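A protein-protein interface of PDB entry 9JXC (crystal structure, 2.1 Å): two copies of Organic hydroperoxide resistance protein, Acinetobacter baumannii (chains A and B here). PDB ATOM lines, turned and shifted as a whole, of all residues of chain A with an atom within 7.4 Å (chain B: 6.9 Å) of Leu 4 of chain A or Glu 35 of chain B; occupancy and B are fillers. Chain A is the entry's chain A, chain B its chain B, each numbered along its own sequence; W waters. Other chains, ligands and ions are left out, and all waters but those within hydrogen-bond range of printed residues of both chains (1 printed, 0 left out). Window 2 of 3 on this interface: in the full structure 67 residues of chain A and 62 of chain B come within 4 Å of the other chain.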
ATOM      1  N   MET A   1     -28.171  23.815 -16.865  1.00  0.00           N
ATOM      2  CA  MET A   1     -28.532  24.242 -15.486  1.00  0.00           C
ATOM      3  C   MET A   1     -27.692  23.493 -14.439  1.00  0.00           C
ATOM      4  O   MET A   1     -26.882  24.157 -13.790  1.00  0.00           O
ATOM      5  CB  MET A   1     -30.033  24.076 -15.198  1.00  0.00           C
ATOM      6  CG  MET A   1     -30.639  22.737 -15.574  1.00  0.00           C
ATOM      7  SD  MET A   1     -31.034  21.705 -14.160  1.00  0.00           S
ATOM      8  CE  MET A   1     -32.178  22.759 -13.263  1.00  0.00           C
ATOM      9  N   SER A   2     -27.866  22.176 -14.295  1.00  0.00           N
ATOM     10  CA  SER A   2     -27.349  21.345 -13.176  1.00  0.00           C
ATOM     11  C   SER A   2     -25.897  21.696 -12.800  1.00  0.00           C
ATOM     12  O   SER A   2     -25.055  21.806 -13.686  1.00  0.00           O
ATOM     13  CB  SER A   2     -27.450  19.865 -13.520  1.00  0.00           C
ATOM     14  OG  SER A   2     -28.484  19.248 -12.780  1.00  0.00           O
ATOM     15  N   THR A   3     -25.590  21.725 -11.504  1.00  0.00           N
ATOM     16  CA  THR A   3     -24.201  21.613 -10.981  1.00  0.00           C
ATOM     17  C   THR A   3     -23.859  20.124 -10.838  1.00  0.00           C
ATOM     18  O   THR A   3     -24.542  19.443 -10.058  1.00  0.00           O
ATOM     19  CB  THR A   3     -24.053  22.342  -9.642  1.00  0.00           C
ATOM     20  OG1 THR A   3     -24.561  23.666  -9.819  1.00  0.00           O
ATOM     21  CG2 THR A   3     -22.617  22.391  -9.157  1.00  0.00           C
ATOM     22  N   LEU A   4     -22.838  19.644 -11.542  1.00  0.00           N
ATOM     23  CA  LEU A   4     -22.444  18.213 -11.553  1.00  0.00           C
ATOM     24  C   LEU A   4     -21.618  17.896 -10.314  1.00  0.00           C
ATOM     25  O   LEU A   4     -21.753  16.779  -9.772  1.00  0.00           O
ATOM     26  CB  LEU A   4     -21.677  17.915 -12.840  1.00  0.00           C
ATOM     27  CG  LEU A   4     -22.483  18.227 -14.107  1.00  0.00           C
ATOM     28  CD1 LEU A   4     -21.795  17.653 -15.331  1.00  0.00           C
ATOM     29  CD2 LEU A   4     -23.916  17.711 -14.009  1.00  0.00           C
ATOM     30  N   TYR A   5     -20.810  18.855  -9.873  1.00  0.00           N
ATOM     31  CA  TYR A   5     -20.003  18.720  -8.648  1.00  0.00           C
ATOM     32  C   TYR A   5     -19.794  20.111  -8.034  1.00  0.00           C
ATOM     33  O   TYR A   5     -19.448  21.065  -8.761  1.00  0.00           O
ATOM     34  CB  TYR A   5     -18.702  17.976  -8.955  1.00  0.00           C
ATOM     35  CG  TYR A   5     -17.747  17.986  -7.794  1.00  0.00           C
ATOM     36  CD1 TYR A   5     -17.921  17.168  -6.689  1.00  0.00           C
ATOM     37  CD2 TYR A   5     -16.665  18.844  -7.795  1.00  0.00           C
ATOM     38  CE1 TYR A   5     -17.025  17.194  -5.626  1.00  0.00           C
ATOM     39  CE2 TYR A   5     -15.788  18.905  -6.731  1.00  0.00           C
ATOM     40  CZ  TYR A   5     -15.959  18.080  -5.636  1.00  0.00           C
ATOM     41  OH  TYR A   5     -15.036  18.169  -4.614  1.00  0.00           O
ATOM     42  N   SER A   6     -19.971  20.198  -6.723  1.00  0.00           N
ATOM     43  CA  SER A   6     -19.816  21.446  -5.933  1.00  0.00           C
ATOM     44  C   SER A   6     -19.023  21.139  -4.675  1.00  0.00           C
ATOM     45  O   SER A   6     -19.204  20.017  -4.099  1.00  0.00           O
ATOM     46  CB  SER A   6     -21.141  22.057  -5.607  1.00  0.00           C
ATOM     47  OG  SER A   6     -20.949  23.284  -4.927  1.00  0.00           O
ATOM     48  N   LEU B  32     -10.675  12.072  -8.891  1.00  0.00           N
ATOM     49  CA  LEU B  32     -12.000  12.409  -9.457  1.00  0.00           C
ATOM     50  C   LEU B  32     -13.015  12.295  -8.332  1.00  0.00           C
ATOM     51  O   LEU B  32     -13.100  11.248  -7.690  1.00  0.00           O
ATOM     52  CB  LEU B  32     -12.409  11.420 -10.552  1.00  0.00           C
ATOM     53  CG  LEU B  32     -11.991  11.722 -11.981  1.00  0.00           C
ATOM     54  CD1 LEU B  32     -12.775  10.813 -12.913  1.00  0.00           C
ATOM     55  CD2 LEU B  32     -12.185  13.188 -12.350  1.00  0.00           C
ATOM     56  N   PRO B  33     -13.865  13.320  -8.104  1.00  0.00           N
ATOM     57  CA  PRO B  33     -14.971  13.178  -7.167  1.00  0.00           C
ATOM     58  C   PRO B  33     -15.936  12.054  -7.595  1.00  0.00           C
ATOM     59  O   PRO B  33     -15.933  11.605  -8.732  1.00  0.00           O
ATOM     60  CB  PRO B  33     -15.639  14.560  -7.159  1.00  0.00           C
ATOM     61  CG  PRO B  33     -15.150  15.253  -8.413  1.00  0.00           C
ATOM     62  CD  PRO B  33     -13.785  14.667  -8.702  1.00  0.00           C
ATOM     63  N   LYS B  34     -16.718  11.579  -6.640  1.00  0.00           N
ATOM     64  CA  LYS B  34     -17.627  10.427  -6.839  1.00  0.00           C
ATOM     65  C   LYS B  34     -18.676  10.834  -7.877  1.00  0.00           C
ATOM     66  O   LYS B  34     -19.087   9.959  -8.660  1.00  0.00           O
ATOM     67  CB  LYS B  34     -18.246  10.008  -5.508  1.00  0.00           C
ATOM     68  CG  LYS B  34     -17.371   9.089  -4.669  1.00  0.00           C
ATOM     69  CD  LYS B  34     -17.745   9.106  -3.203  1.00  0.00           C
ATOM     70  CE  LYS B  34     -17.411   7.824  -2.467  1.00  0.00           C
ATOM     71  NZ  LYS B  34     -17.480   8.030  -1.000  1.00  0.00           N
ATOM     72  N   GLU B  35     -19.043  12.123  -7.908  1.00  0.00           N
ATOM     73  CA  GLU B  35     -20.074  12.657  -8.820  1.00  0.00           C
ATOM     74  C   GLU B  35     -19.582  12.476 -10.259  1.00  0.00           C
ATOM     75  O   GLU B  35     -20.441  12.398 -11.143  1.00  0.00           O
ATOM     76  CB  GLU B  35     -20.410  14.110  -8.499  1.00  0.00           C
ATOM     77  CG  GLU B  35     -21.085  14.311  -7.159  1.00  0.00           C
ATOM     78  CD  GLU B  35     -20.167  14.467  -5.956  1.00  0.00           C
ATOM     79  OE1 GLU B  35     -19.001  14.001  -5.991  1.00  0.00           O
ATOM     80  OE2 GLU B  35     -20.618  15.063  -4.970  1.00  0.00           O
ATOM     81  N   LEU B  36     -18.265  12.363 -10.472  1.00  0.00           N
ATOM     82  CA  LEU B  36     -17.663  12.136 -11.820  1.00  0.00           C
ATOM     83  C   LEU B  36     -17.114  10.714 -11.908  1.00  0.00           C
ATOM     84  O   LEU B  36     -16.279  10.458 -12.783  1.00  0.00           O
ATOM     85  CB  LEU B  36     -16.567  13.180 -12.086  1.00  0.00           C
ATOM     86  CG  LEU B  36     -17.027  14.629 -11.924  1.00  0.00           C
ATOM     87  CD1 LEU B  36     -15.865  15.621 -12.048  1.00  0.00           C
ATOM     88  CD2 LEU B  36     -18.130  14.951 -12.923  1.00  0.00           C
ATOM     89  N   GLY B  37     -17.593   9.823 -11.043  1.00  0.00           N
ATOM     90  CA  GLY B  37     -17.316   8.376 -11.144  1.00  0.00           C
ATOM     91  C   GLY B  37     -15.945   8.006 -10.604  1.00  0.00           C
ATOM     92  O   GLY B  37     -15.507   6.880 -10.878  1.00  0.00           O
ATOM     93  N   GLY B  38     -15.302   8.895  -9.833  1.00  0.00           N
ATOM     94  CA  GLY B  38     -14.042   8.610  -9.110  1.00  0.00           C
ATOM     95  C   GLY B  38     -14.309   8.163  -7.690  1.00  0.00           C
ATOM     96  O   GLY B  38     -15.462   8.052  -7.344  1.00  0.00           O
ATOM     97  N   GLY B  40     -13.418   9.906  -4.849  1.00  0.00           N
ATOM     98  CA  GLY B  40     -13.602  11.032  -3.901  1.00  0.00           C
ATOM     99  C   GLY B  40     -12.651  10.916  -2.712  1.00  0.00           C
ATOM    100  O   GLY B  40     -12.981  11.381  -1.627  1.00  0.00           O
ATOM    101  N   GLY B  85     -18.290  25.200  -8.093  1.00  0.00           N
ATOM    102  CA  GLY B  85     -18.979  24.118  -8.810  1.00  0.00           C
ATOM    103  C   GLY B  85     -18.461  23.998 -10.220  1.00  0.00           C
ATOM    104  O   GLY B  85     -17.677  24.882 -10.683  1.00  0.00           O
ATOM    105  N   ILE B  86     -18.925  22.949 -10.873  1.00  0.00           N
ATOM    106  CA  ILE B  86     -18.595  22.601 -12.268  1.00  0.00           C
ATOM    107  C   ILE B  86     -19.925  22.330 -12.976  1.00  0.00           C
ATOM    108  O   ILE B  86     -20.715  21.506 -12.474  1.00  0.00           O
ATOM    109  CB  ILE B  86     -17.571  21.448 -12.255  1.00  0.00           C
ATOM    110  CG1 ILE B  86     -16.807  21.366 -13.566  1.00  0.00           C
ATOM    111  CG2 ILE B  86     -18.167  20.117 -11.859  1.00  0.00           C
ATOM    112  CD1 ILE B  86     -15.422  21.966 -13.460  1.00  0.00           C
ATOM    113  N   VAL B  87     -20.231  23.115 -14.000  1.00  0.00           N
ATOM    114  CA  VAL B  87     -21.500  22.986 -14.783  1.00  0.00           C
ATOM    115  C   VAL B  87     -21.135  22.548 -16.210  1.00  0.00           C
ATOM    116  O   VAL B  87     -20.104  23.012 -16.738  1.00  0.00           O
ATOM    117  CB  VAL B  87     -22.343  24.276 -14.775  1.00  0.00           C
ATOM    118  CG1 VAL B  87     -22.814  24.650 -13.377  1.00  0.00           C
ATOM    119  CG2 VAL B  87     -21.626  25.448 -15.404  1.00  0.00           C
ATOM    120  N   ALA B  88     -21.928  21.666 -16.819  1.00  0.00           N
ATOM    121  CA  ALA B  88     -21.702  21.221 -18.215  1.00  0.00           C
ATOM    122  C   ALA B  88     -21.950  22.409 -19.151  1.00  0.00           C
ATOM    123  O   ALA B  88     -22.949  23.111 -18.942  1.00  0.00           O
ATOM    124  CB  ALA B  88     -22.595  20.043 -18.531  1.00  0.00           C
ATOM    125  N   GLY B  93     -17.882  19.980 -22.442  1.00  0.00           N
ATOM    126  CA  GLY B  93     -16.880  20.321 -21.412  1.00  0.00           C
ATOM    127  C   GLY B  93     -17.550  20.916 -20.182  1.00  0.00           C
ATOM    128  O   GLY B  93     -18.808  20.862 -20.101  1.00  0.00           O
ATOM    129  N   PHE B  94     -16.742  21.455 -19.260  1.00  0.00           N
ATOM    130  CA  PHE B  94     -17.159  22.039 -17.959  1.00  0.00           C
ATOM    131  C   PHE B  94     -16.801  23.539 -17.909  1.00  0.00           C
ATOM    132  O   PHE B  94     -15.811  23.937 -18.555  1.00  0.00           O
ATOM    133  CB  PHE B  94     -16.447  21.329 -16.808  1.00  0.00           C
ATOM    134  CG  PHE B  94     -16.718  19.849 -16.628  1.00  0.00           C
ATOM    135  CD1 PHE B  94     -18.012  19.362 -16.480  1.00  0.00           C
ATOM    136  CD2 PHE B  94     -15.666  18.944 -16.496  1.00  0.00           C
ATOM    137  CE1 PHE B  94     -18.241  18.005 -16.270  1.00  0.00           C
ATOM    138  CE2 PHE B  94     -15.899  17.588 -16.291  1.00  0.00           C
ATOM    139  CZ  PHE B  94     -17.187  17.119 -16.184  1.00  0.00           C
HETATM  140  O   HOH W   1     -21.333  17.887  -5.491  1.00  0.00           O
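N of Leu 4 of chain A is in hydrogen-bond range of O of Ile 86 of chain B (3.0 Å).
The backbone NH of Ile 86 of chain B lies within hydrogen-bond range of the backbone carbonyl oxygen of Tyr 5 of chain A (2.9 Å).
Printed residues of chain B within 4 Å of Ser 2 of chain A: Val 87 (3.6 Å).
Of the printed residues of chain B, Thr 3 of chain A touches Ile 86.
Printed residues of chain B within 4 Å of Tyr 5 of chain A: Pro 33 (3.3 Å), Glu 35 (3.4 Å), Gly 85 (3.1 Å) and Ile 86 (2.9 Å).
Of chain A, only Leu 4 and Tyr 5 come within 4 Å of Glu 35 of chain B.
Of the printed residues of chain A, Gly 85 of chain B touches Tyr 5.
The nearest residue of chain B that does not touch Leu 4 of chain A is Ala 88 of chain B (4.1 Å).
The nearest residue of chain A that does not touch Glu 35 of chain B is Ser 6 of chain A (5.2 Å).
The nearest printed residue of chain B that does not touch Ser 2 of chain A is Ala 88 of chain B (4.4 Å).
Hydrophobic or aromatic side chains of chain A within 4 Å of the printed part of chain B: Leu 4 and Tyr 5.
Printed residues of chain B that touch a printed residue of chain A: Pro 33, Glu 35, Gly 85, Ile 86, Val 87 and Phe 94.
Hydrophobic or aromatic side chains of chain B that line the printed part of chain A: Pro 33, Ile 86, Val 87 and Phe 94.
Among the printed residues, 9 pairs touch across the chains.
Among the printed residues, no Asp or Glu carboxylate lies within 4 Å of a Lys or Arg side-chain nitrogen of the other chain.
O of Ser 2 of chain A touches CG1 of Val 87 of chain B, 3.6 Å away.
CA of Thr 3 of chain A touches O of Ile 86 of chain B (3.8 Å).
Leu 4 of chain A touches Glu 35 of chain B (O to CB, 3.2 Å).
Leu 4 of chain A touches Phe 94 of chain B (CD1 to CE1, 3.7 Å).
CB of Pro 33 of chain B touches CE1 of Tyr 5 of chain A (3.3 Å).
CD1 of Tyr 5 of chain A touches OE1 of Glu 35 of chain B, at 3.4 Å.
Tyr 5 of chain A touches Gly 85 of chain B (O to CA, 3.1 Å).
The backbone NH (N) of Gly 38 of chain B is in hydrogen-bond range of the backbone carbonyl oxygen (O) of Pro 33 of chain B (3.0 Å).
Water W1 lies within hydrogen-bond range of the backbone NH of Ser 6 of chain A (3.0 Å) and the side-chain carboxylate of Glu 35 of chain B (3.0 Å).
No position is printed for both chains.
Of the 9 pairs that touch across the chains among the printed residues, none has its exchanged pair printed and touching as well.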
